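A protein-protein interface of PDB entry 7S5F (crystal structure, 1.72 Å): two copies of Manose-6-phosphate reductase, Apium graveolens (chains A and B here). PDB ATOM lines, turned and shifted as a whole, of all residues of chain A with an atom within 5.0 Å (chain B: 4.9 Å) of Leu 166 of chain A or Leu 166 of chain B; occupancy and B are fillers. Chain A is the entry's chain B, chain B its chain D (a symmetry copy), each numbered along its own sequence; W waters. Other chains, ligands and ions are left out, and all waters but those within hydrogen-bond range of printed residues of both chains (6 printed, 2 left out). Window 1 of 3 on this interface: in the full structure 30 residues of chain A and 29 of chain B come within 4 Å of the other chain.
Printed residues of chain B that touch a printed residue of chain A: Pro 109, Leu 138, Asp 163, Tyr 165, Leu 166, Arg 168 and Asp 169. Hydrophobic or aromatic side chains of chain B that line the printed part of chain A: Pro 109, Leu 138, Tyr 165 and Leu 166. Among the printed residues, no Asp or Glu carboxylate lies within 4 Å of a Lys or Arg side-chain nitrogen of the other chain.
The side-chain carboxylate (OD1) of Asp 169 of chain B is in hydrogen-bond range of the backbone NH (N) of Leu 138 of chain A, at 2.7 Å. The side-chain carboxylate (OD1) of Asp 169 of chain A sits at hydrogen-bond distance from the backbone NH (N) of Leu 138 of chain B.
Of chain B, only Leu 166 comes within 4 Å of Leu 166 of chain A. Leu 166 of chain B touches just one residue of chain A: Leu 166. Printed residues of chain B within 4 Å of Pro 109 of chain A: Tyr 165. Of the printed residues of chain B, Arg 168 of chain A touches Leu 138 (3.8 Å). Of the printed residues of chain A, Pro 109 of chain B touches Tyr 165 (3.2 Å). Printed residues of chain A within 4 Å of Leu 138 of chain B: Arg 168 (3.8 Å) and Asp 169 (2.8 Å). Asn 161 of chain A touches none of the printed residues of chain B. The nearest residue of chain B that does not touch Leu 166 of chain A is Tyr 165 of chain B (4.1 Å). The nearest residue of chain A that does not touch Leu 166 of chain B is Tyr 165 of chain A (4.1 Å). The nearest printed residue of chain B that does not touch Arg 168 of chain A is Pro 109 of chain B (4.3 Å).
Leu 138 of chain A touches Arg 168 of chain B, and with the chains exchanged Arg 168 of chain A touches Leu 138 of chain B. Leu 138 of chain A touches Asp 169 of chain B, and with the chains exchanged Asp 169 of chain A touches Leu 138 of chain B. Asp 163 of chain B touches its own counterpart, Asp 163 of chain A. Leu 166 of chain A touches its own counterpart, Leu 166 of chain B. Of the 8 pairs that touch across the chains among the printed residues, 8 have their exchanged pair printed and touching as well.
The side-chain carboxylate (OD1) of Asp 163 of chain A lies close to the backbone NH (N) of Tyr 165 of chain A. The backbone carbonyl oxygen (O) of Asp 163 of chain A is in hydrogen-bond range of the side-chain hydroxyl (OG1) of Thr 167 of chain A (2.7 Å). NH2 of Arg 168 of chain A is in salt-bridge range of OD1 of Asp 169 of chain A, 3.3 Å away. The side-chain carboxylate (OD1) of Asp 163 of chain B sits at hydrogen-bond distance from the backbone NH (N) of Tyr 165 of chain B (3.2 Å). The side-chain carboxylate of Asp 163 of chain B lies within hydrogen-bond range of the backbone NH of Leu 166 of chain B, 2.8 Å away. The side-chain carboxylate (OD1) of Asp 169 of chain B lies within salt-bridge range of the guanidinium group (NH2) of Arg 168 of chain B.
Water W6 lies within hydrogen-bond range of OD2 of Asp 169 of chain B (2.6 Å) and OD2 of Asp 169 of chain A (2.8 Å). Water W2 lies within hydrogen-bond range of the backbone carbonyl oxygen (O) of Pro 109 of chain B (2.7 Å), the backbone carbonyl oxygen (O) of Tyr 165 of chain A (2.7 Å) and the guanidinium group (NE) of Arg 168 of chain A (2.9 Å). Water W4 lies within hydrogen-bond range of OD2 of Asp 169 of chain B and N of Leu 138 of chain A. Water W5 lies within hydrogen-bond range of the side-chain carboxylate of Asp 169 of chain A (2.7 Å) and the backbone NH of Leu 138 of chain B (3.4 Å). Water W1 lies within hydrogen-bond range of the guanidinium group (NE) of Arg 168 of chain B, the backbone carbonyl oxygen (O) of Pro 109 of chain A and the backbone carbonyl oxygen (O) of Tyr 165 of chain B. Water W3 bridges OD2 of Asp 169 of chain A (2.8 Å) and OD2 of Asp 169 of chain B (2.8 Å).
CD1 of Tyr 165 of chain B touches O of Pro 109 of chain A, at 3.1 Å. NH2 of Arg 168 of chain B touches CD2 of Leu 138 of chain A (3.7 Å). Asp 163 of chain A touches Asp 163 of chain B. Pro 109 of chain B touches Tyr 165 of chain A. Leu 166 of chain B touches Leu 166 of chain A (CD2 to CD2, 3.7 Å). NH2 of Arg 168 of chain A touches CD2 of Leu 138 of chain B, at 3.8 Å.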
ATOM      1  N   PRO A 109     -23.174 -16.169  16.945  1.00  0.00           N
ATOM      2  CA  PRO A 109     -22.221 -16.038  15.835  1.00  0.00           C
ATOM      3  C   PRO A 109     -22.640 -16.864  14.618  1.00  0.00           C
ATOM      4  O   PRO A 109     -21.830 -17.548  13.993  1.00  0.00           O
ATOM      5  CB  PRO A 109     -20.914 -16.540  16.454  1.00  0.00           C
ATOM      6  CG  PRO A 109     -21.374 -17.596  17.426  1.00  0.00           C
ATOM      7  CD  PRO A 109     -22.646 -17.033  18.022  1.00  0.00           C
ATOM      8  N   LEU A 138     -19.354 -12.028  10.304  1.00  0.00           N
ATOM      9  CA  LEU A 138     -19.623 -11.489  11.636  1.00  0.00           C
ATOM     10  C   LEU A 138     -19.092 -10.068  11.774  1.00  0.00           C
ATOM     11  O   LEU A 138     -19.700  -9.241  12.461  1.00  0.00           O
ATOM     12  CB  LEU A 138     -19.009 -12.395  12.705  1.00  0.00           C
ATOM     13  CG  LEU A 138     -19.631 -13.799  12.752  1.00  0.00           C
ATOM     14  CD1 LEU A 138     -18.959 -14.670  13.814  1.00  0.00           C
ATOM     15  CD2 LEU A 138     -21.138 -13.715  12.998  1.00  0.00           C
ATOM     16  N   ASN A 161     -22.772 -15.793  23.061  1.00  0.00           N
ATOM     17  CA  ASN A 161     -22.350 -17.135  22.663  1.00  0.00           C
ATOM     18  C   ASN A 161     -21.102 -17.106  21.784  1.00  0.00           C
ATOM     19  O   ASN A 161     -20.918 -17.972  20.930  1.00  0.00           O
ATOM     20  CB  ASN A 161     -23.483 -17.878  21.949  1.00  0.00           C
ATOM     21  CG  ASN A 161     -24.733 -17.966  22.798  1.00  0.00           C
ATOM     22  OD1 ASN A 161     -24.698 -18.501  23.902  1.00  0.00           O
ATOM     23  ND2 ASN A 161     -25.840 -17.427  22.295  1.00  0.00           N
ATOM     24  N   TYR A 162     -20.240 -16.105  21.969  1.00  0.00           N
ATOM     25  CA  TYR A 162     -18.935 -16.084  21.314  1.00  0.00           C
ATOM     26  C   TYR A 162     -17.922 -16.778  22.216  1.00  0.00           C
ATOM     27  O   TYR A 162     -17.821 -16.460  23.409  1.00  0.00           O
ATOM     28  CB  TYR A 162     -18.473 -14.654  21.028  1.00  0.00           C
ATOM     29  CG  TYR A 162     -19.095 -13.994  19.818  1.00  0.00           C
ATOM     30  CD1 TYR A 162     -20.465 -14.069  19.569  1.00  0.00           C
ATOM     31  CD2 TYR A 162     -18.313 -13.261  18.941  1.00  0.00           C
ATOM     32  CE1 TYR A 162     -21.030 -13.436  18.462  1.00  0.00           C
ATOM     33  CE2 TYR A 162     -18.860 -12.630  17.841  1.00  0.00           C
ATOM     34  CZ  TYR A 162     -20.212 -12.711  17.603  1.00  0.00           C
ATOM     35  OH  TYR A 162     -20.738 -12.069  16.496  1.00  0.00           O
ATOM     36  N   ASP A 163     -17.178 -17.723  21.647  1.00  0.00           N
ATOM     37  CA  ASP A 163     -16.152 -18.451  22.377  1.00  0.00           C
ATOM     38  C   ASP A 163     -14.837 -17.673  22.340  1.00  0.00           C
ATOM     39  O   ASP A 163     -14.795 -16.514  21.917  1.00  0.00           O
ATOM     40  CB  ASP A 163     -16.024 -19.861  21.812  1.00  0.00           C
ATOM     41  CG  ASP A 163     -15.558 -19.875  20.363  1.00  0.00           C
ATOM     42  OD1 ASP A 163     -15.301 -18.795  19.788  1.00  0.00           O
ATOM     43  OD2 ASP A 163     -15.493 -20.977  19.785  1.00  0.00           O
ATOM     44  N   VAL A 164     -13.746 -18.301  22.793  1.00  0.00           N
ATOM     45  CA  VAL A 164     -12.459 -17.600  22.852  1.00  0.00           C
ATOM     46  C   VAL A 164     -12.016 -17.171  21.457  1.00  0.00           C
ATOM     47  O   VAL A 164     -11.544 -16.044  21.260  1.00  0.00           O
ATOM     48  CB  VAL A 164     -11.389 -18.471  23.538  1.00  0.00           C
ATOM     49  CG1 VAL A 164      -9.989 -17.928  23.235  1.00  0.00           C
ATOM     50  CG2 VAL A 164     -11.624 -18.538  25.055  1.00  0.00           C
ATOM     51  N   TYR A 165     -12.161 -18.053  20.464  1.00  0.00           N
ATOM     52  CA  TYR A 165     -11.697 -17.718  19.123  1.00  0.00           C
ATOM     53  C   TYR A 165     -12.498 -16.568  18.534  1.00  0.00           C
ATOM     54  O   TYR A 165     -11.935 -15.642  17.936  1.00  0.00           O
ATOM     55  CB  TYR A 165     -11.804 -18.933  18.209  1.00  0.00           C
ATOM     56  CG  TYR A 165     -10.859 -20.068  18.505  1.00  0.00           C
ATOM     57  CD1 TYR A 165      -9.516 -19.836  18.755  1.00  0.00           C
ATOM     58  CD2 TYR A 165     -11.313 -21.382  18.488  1.00  0.00           C
ATOM     59  CE1 TYR A 165      -8.647 -20.883  19.001  1.00  0.00           C
ATOM     60  CE2 TYR A 165     -10.452 -22.436  18.729  1.00  0.00           C
ATOM     61  CZ  TYR A 165      -9.120 -22.180  18.980  1.00  0.00           C
ATOM     62  OH  TYR A 165      -8.274 -23.234  19.211  1.00  0.00           O
ATOM     63  N   LEU A 166     -13.822 -16.625  18.674  1.00  0.00           N
ATOM     64  CA  LEU A 166     -14.663 -15.583  18.097  1.00  0.00           C
ATOM     65  C   LEU A 166     -14.490 -14.265  18.837  1.00  0.00           C
ATOM     66  O   LEU A 166     -14.533 -13.195  18.219  1.00  0.00           O
ATOM     67  CB  LEU A 166     -16.127 -16.024  18.108  1.00  0.00           C
ATOM     68  CG  LEU A 166     -16.439 -17.185  17.165  1.00  0.00           C
ATOM     69  CD1 LEU A 166     -17.725 -17.879  17.597  1.00  0.00           C
ATOM     70  CD2 LEU A 166     -16.545 -16.690  15.726  1.00  0.00           C
ATOM     71  N   THR A 167     -14.285 -14.322  20.157  1.00  0.00           N
ATOM     72  CA  THR A 167     -14.055 -13.098  20.917  1.00  0.00           C
ATOM     73  C   THR A 167     -12.725 -12.462  20.533  1.00  0.00           C
ATOM     74  O   THR A 167     -12.639 -11.236  20.386  1.00  0.00           O
ATOM     75  CB  THR A 167     -14.105 -13.378  22.422  1.00  0.00           C
ATOM     76  OG1 THR A 167     -15.365 -13.977  22.757  1.00  0.00           O
ATOM     77  CG2 THR A 167     -13.964 -12.081  23.211  1.00  0.00           C
ATOM     78  N   ARG A 168     -11.680 -13.273  20.354  1.00  0.00           N
ATOM     79  CA  ARG A 168     -10.412 -12.717  19.892  1.00  0.00           C
ATOM     80  C   ARG A 168     -10.567 -12.057  18.529  1.00  0.00           C
ATOM     81  O   ARG A 168      -9.952 -11.018  18.259  1.00  0.00           O
ATOM     82  CB  ARG A 168      -9.336 -13.801  19.824  1.00  0.00           C
ATOM     83  CG  ARG A 168      -7.940 -13.223  19.596  1.00  0.00           C
ATOM     84  CD  ARG A 168      -7.015 -14.127  18.766  1.00  0.00           C
ATOM     85  NE  ARG A 168      -7.521 -14.265  17.410  1.00  0.00           N
ATOM     86  CZ  ARG A 168      -7.308 -13.390  16.437  1.00  0.00           C
ATOM     87  NH1 ARG A 168      -6.496 -12.354  16.601  1.00  0.00           N
ATOM     88  NH2 ARG A 168      -7.945 -13.541  15.279  1.00  0.00           N
ATOM     89  N   ASP A 169     -11.384 -12.646  17.655  1.00  0.00           N
ATOM     90  CA  ASP A 169     -11.553 -12.081  16.319  1.00  0.00           C
ATOM     91  C   ASP A 169     -12.244 -10.719  16.375  1.00  0.00           C
ATOM     92  O   ASP A 169     -11.798  -9.767  15.729  1.00  0.00           O
ATOM     93  CB  ASP A 169     -12.326 -13.052  15.429  1.00  0.00           C
ATOM     94  CG  ASP A 169     -11.876 -12.997  13.977  1.00  0.00           C
ATOM     95  OD1 ASP A 169     -10.726 -12.593  13.710  1.00  0.00           O
ATOM     96  OD2 ASP A 169     -12.674 -13.361  13.091  1.00  0.00           O
ATOM     97  N   ILE A 170     -13.328 -10.600  17.149  1.00  0.00           N
ATOM     98  CA  ILE A 170     -14.008  -9.305  17.206  1.00  0.00           C
ATOM     99  C   ILE A 170     -13.147  -8.269  17.931  1.00  0.00           C
ATOM    100  O   ILE A 170     -13.169  -7.086  17.575  1.00  0.00           O
ATOM    101  CB  ILE A 170     -15.415  -9.433  17.829  1.00  0.00           C
ATOM    102  CG1 ILE A 170     -16.114  -8.069  17.822  1.00  0.00           C
ATOM    103  CG2 ILE A 170     -15.354  -9.982  19.253  1.00  0.00           C
ATOM    104  CD1 ILE A 170     -17.571  -8.112  18.260  1.00  0.00           C
ATOM    105  N   PRO B 109      -7.403 -21.069  14.372  1.00  0.00           N
ATOM    106  CA  PRO B 109      -8.072 -19.758  14.367  1.00  0.00           C
ATOM    107  C   PRO B 109      -7.655 -18.898  15.550  1.00  0.00           C
ATOM    108  O   PRO B 109      -8.491 -18.267  16.207  1.00  0.00           O
ATOM    109  CB  PRO B 109      -9.555 -20.128  14.444  1.00  0.00           C
ATOM    110  CG  PRO B 109      -9.559 -21.421  15.232  1.00  0.00           C
ATOM    111  CD  PRO B 109      -8.313 -22.157  14.775  1.00  0.00           C
ATOM    112  N   LEU B 138      -8.886 -12.949  11.627  1.00  0.00           N
ATOM    113  CA  LEU B 138      -8.770 -14.134  10.785  1.00  0.00           C
ATOM    114  C   LEU B 138      -9.000 -13.784   9.319  1.00  0.00           C
ATOM    115  O   LEU B 138      -8.358 -14.357   8.433  1.00  0.00           O
ATOM    116  CB  LEU B 138      -9.754 -15.216  11.239  1.00  0.00           C
ATOM    117  CG  LEU B 138      -9.510 -15.762  12.656  1.00  0.00           C
ATOM    118  CD1 LEU B 138     -10.569 -16.782  13.036  1.00  0.00           C
ATOM    119  CD2 LEU B 138      -8.108 -16.363  12.788  1.00  0.00           C
ATOM    120  N   ASN B 161      -8.755 -26.669  12.194  1.00  0.00           N
ATOM    121  CA  ASN B 161      -9.422 -26.529  13.490  1.00  0.00           C
ATOM    122  C   ASN B 161     -10.442 -25.392  13.501  1.00  0.00           C
ATOM    123  O   ASN B 161     -10.632 -24.734  14.525  1.00  0.00           O
ATOM    124  CB  ASN B 161      -8.402 -26.336  14.618  1.00  0.00           C
ATOM    125  CG  ASN B 161      -7.369 -27.438  14.654  1.00  0.00           C
ATOM    126  OD1 ASN B 161      -7.709 -28.611  14.780  1.00  0.00           O
ATOM    127  ND2 ASN B 161      -6.103 -27.069  14.536  1.00  0.00           N
ATOM    128  N   TYR B 162     -11.114 -25.154  12.371  1.00  0.00           N
ATOM    129  CA  TYR B 162     -12.223 -24.210  12.319  1.00  0.00           C
ATOM    130  C   TYR B 162     -13.529 -24.959  12.568  1.00  0.00           C
ATOM    131  O   TYR B 162     -13.785 -25.992  11.938  1.00  0.00           O
ATOM    132  CB  TYR B 162     -12.266 -23.500  10.961  1.00  0.00           C
ATOM    133  CG  TYR B 162     -11.312 -22.322  10.771  1.00  0.00           C
ATOM    134  CD1 TYR B 162      -9.979 -22.392  11.172  1.00  0.00           C
ATOM    135  CD2 TYR B 162     -11.746 -21.152  10.148  1.00  0.00           C
ATOM    136  CE1 TYR B 162      -9.110 -21.321  10.973  1.00  0.00           C
ATOM    137  CE2 TYR B 162     -10.891 -20.080   9.947  1.00  0.00           C
ATOM    138  CZ  TYR B 162      -9.577 -20.168  10.358  1.00  0.00           C
ATOM    139  OH  TYR B 162      -8.729 -19.106  10.155  1.00  0.00           O
ATOM    140  N   ASP B 163     -14.354 -24.453  13.484  1.00  0.00           N
ATOM    141  CA  ASP B 163     -15.619 -25.113  13.783  1.00  0.00           C
ATOM    142  C   ASP B 163     -16.689 -24.618  12.808  1.00  0.00           C
ATOM    143  O   ASP B 163     -16.382 -23.925  11.837  1.00  0.00           O
ATOM    144  CB  ASP B 163     -16.025 -24.859  15.237  1.00  0.00           C
ATOM    145  CG  ASP B 163     -16.186 -23.372  15.567  1.00  0.00           C
ATOM    146  OD1 ASP B 163     -16.102 -22.511  14.669  1.00  0.00           O
ATOM    147  OD2 ASP B 163     -16.393 -23.055  16.747  1.00  0.00           O
ATOM    148  N   VAL B 164     -17.959 -24.922  13.087  1.00  0.00           N
ATOM    149  CA  VAL B 164     -19.034 -24.521  12.183  1.00  0.00           C
ATOM    150  C   VAL B 164     -19.106 -23.002  12.081  1.00  0.00           C
ATOM    151  O   VAL B 164     -19.256 -22.439  10.986  1.00  0.00           O
ATOM    152  CB  VAL B 164     -20.381 -25.118  12.636  1.00  0.00           C
ATOM    153  CG1 VAL B 164     -21.554 -24.418  11.938  1.00  0.00           C
ATOM    154  CG2 VAL B 164     -20.426 -26.623  12.369  1.00  0.00           C
ATOM    155  N   TYR B 165     -19.001 -22.316  13.219  1.00  0.00           N
ATOM    156  CA  TYR B 165     -19.130 -20.861  13.229  1.00  0.00           C
ATOM    157  C   TYR B 165     -17.997 -20.209  12.450  1.00  0.00           C
ATOM    158  O   TYR B 165     -18.223 -19.292  11.648  1.00  0.00           O
ATOM    159  CB  TYR B 165     -19.130 -20.355  14.665  1.00  0.00           C
ATOM    160  CG  TYR B 165     -20.364 -20.656  15.491  1.00  0.00           C
ATOM    161  CD1 TYR B 165     -21.640 -20.531  14.959  1.00  0.00           C
ATOM    162  CD2 TYR B 165     -20.241 -21.020  16.824  1.00  0.00           C
ATOM    163  CE1 TYR B 165     -22.762 -20.784  15.738  1.00  0.00           C
ATOM    164  CE2 TYR B 165     -21.346 -21.279  17.602  1.00  0.00           C
ATOM    165  CZ  TYR B 165     -22.605 -21.155  17.060  1.00  0.00           C
ATOM    166  OH  TYR B 165     -23.699 -21.394  17.853  1.00  0.00           O
ATOM    167  N   LEU B 166     -16.759 -20.650  12.694  1.00  0.00           N
ATOM    168  CA  LEU B 166     -15.628 -20.027  12.022  1.00  0.00           C
ATOM    169  C   LEU B 166     -15.619 -20.375  10.546  1.00  0.00           C
ATOM    170  O   LEU B 166     -15.177 -19.560   9.724  1.00  0.00           O
ATOM    171  CB  LEU B 166     -14.313 -20.456  12.668  1.00  0.00           C
ATOM    172  CG  LEU B 166     -14.107 -19.938  14.096  1.00  0.00           C
ATOM    173  CD1 LEU B 166     -13.070 -20.812  14.780  1.00  0.00           C
ATOM    174  CD2 LEU B 166     -13.703 -18.472  14.108  1.00  0.00           C
ATOM    175  N   THR B 167     -16.121 -21.568  10.193  1.00  0.00           N
ATOM    176  CA  THR B 167     -16.158 -21.968   8.790  1.00  0.00           C
ATOM    177  C   THR B 167     -17.204 -21.165   8.033  1.00  0.00           C
ATOM    178  O   THR B 167     -16.966 -20.747   6.891  1.00  0.00           O
ATOM    179  CB  THR B 167     -16.435 -23.475   8.661  1.00  0.00           C
ATOM    180  OG1 THR B 167     -15.396 -24.239   9.296  1.00  0.00           O
ATOM    181  CG2 THR B 167     -16.522 -23.881   7.190  1.00  0.00           C
ATOM    182  N   ARG B 168     -18.367 -20.931   8.654  1.00  0.00           N
ATOM    183  CA  ARG B 168     -19.371 -20.079   8.028  1.00  0.00           C
ATOM    184  C   ARG B 168     -18.824 -18.680   7.795  1.00  0.00           C
ATOM    185  O   ARG B 168     -19.104 -18.053   6.764  1.00  0.00           O
ATOM    186  CB  ARG B 168     -20.627 -20.006   8.890  1.00  0.00           C
ATOM    187  CG  ARG B 168     -21.811 -19.353   8.164  1.00  0.00           C
ATOM    188  CD  ARG B 168     -22.741 -18.570   9.092  1.00  0.00           C
ATOM    189  NE  ARG B 168     -22.070 -17.420   9.675  1.00  0.00           N
ATOM    190  CZ  ARG B 168     -21.922 -16.251   9.067  1.00  0.00           C
ATOM    191  NH1 ARG B 168     -22.465 -16.013   7.882  1.00  0.00           N
ATOM    192  NH2 ARG B 168     -21.203 -15.301   9.655  1.00  0.00           N
ATOM    193  N   ASP B 169     -18.044 -18.173   8.752  1.00  0.00           N
ATOM    194  CA  ASP B 169     -17.501 -16.827   8.638  1.00  0.00           C
ATOM    195  C   ASP B 169     -16.534 -16.724   7.464  1.00  0.00           C
ATOM    196  O   ASP B 169     -16.653 -15.815   6.638  1.00  0.00           O
ATOM    197  CB  ASP B 169     -16.826 -16.418   9.951  1.00  0.00           C
ATOM    198  CG  ASP B 169     -16.975 -14.930  10.246  1.00  0.00           C
ATOM    199  OD1 ASP B 169     -17.944 -14.309   9.748  1.00  0.00           O
ATOM    200  OD2 ASP B 169     -16.124 -14.380  10.975  1.00  0.00           O
ATOM    201  N   ILE B 170     -15.583 -17.661   7.355  1.00  0.00           N
ATOM    202  CA  ILE B 170     -14.644 -17.578   6.237  1.00  0.00           C
ATOM    203  C   ILE B 170     -15.360 -17.791   4.914  1.00  0.00           C
ATOM    204  O   ILE B 170     -15.011 -17.165   3.909  1.00  0.00           O
ATOM    205  CB  ILE B 170     -13.456 -18.552   6.397  1.00  0.00           C
ATOM    206  CG1 ILE B 170     -12.524 -18.421   5.191  1.00  0.00           C
ATOM    207  CG2 ILE B 170     -13.917 -20.008   6.509  1.00  0.00           C
ATOM    208  CD1 ILE B 170     -11.175 -19.106   5.376  1.00  0.00           C
HETATM  209  O   HOH W   1     -20.310 -17.430  11.742  1.00  0.00           O
HETATM  210  O   HOH W   2      -9.681 -15.902  16.461  1.00  0.00           O
HETATM  211  O   HOH W   3     -15.409 -13.652  13.612  1.00  0.00           O
HETATM  212  O   HOH W   4     -16.203 -11.783  10.381  1.00  0.00           O
HETATM  213  O   HOH W   5     -12.070 -12.160  10.755  1.00  0.00           O
HETATM  214  O   HOH W   6     -13.868 -15.428  11.649  1.00  0.00           O
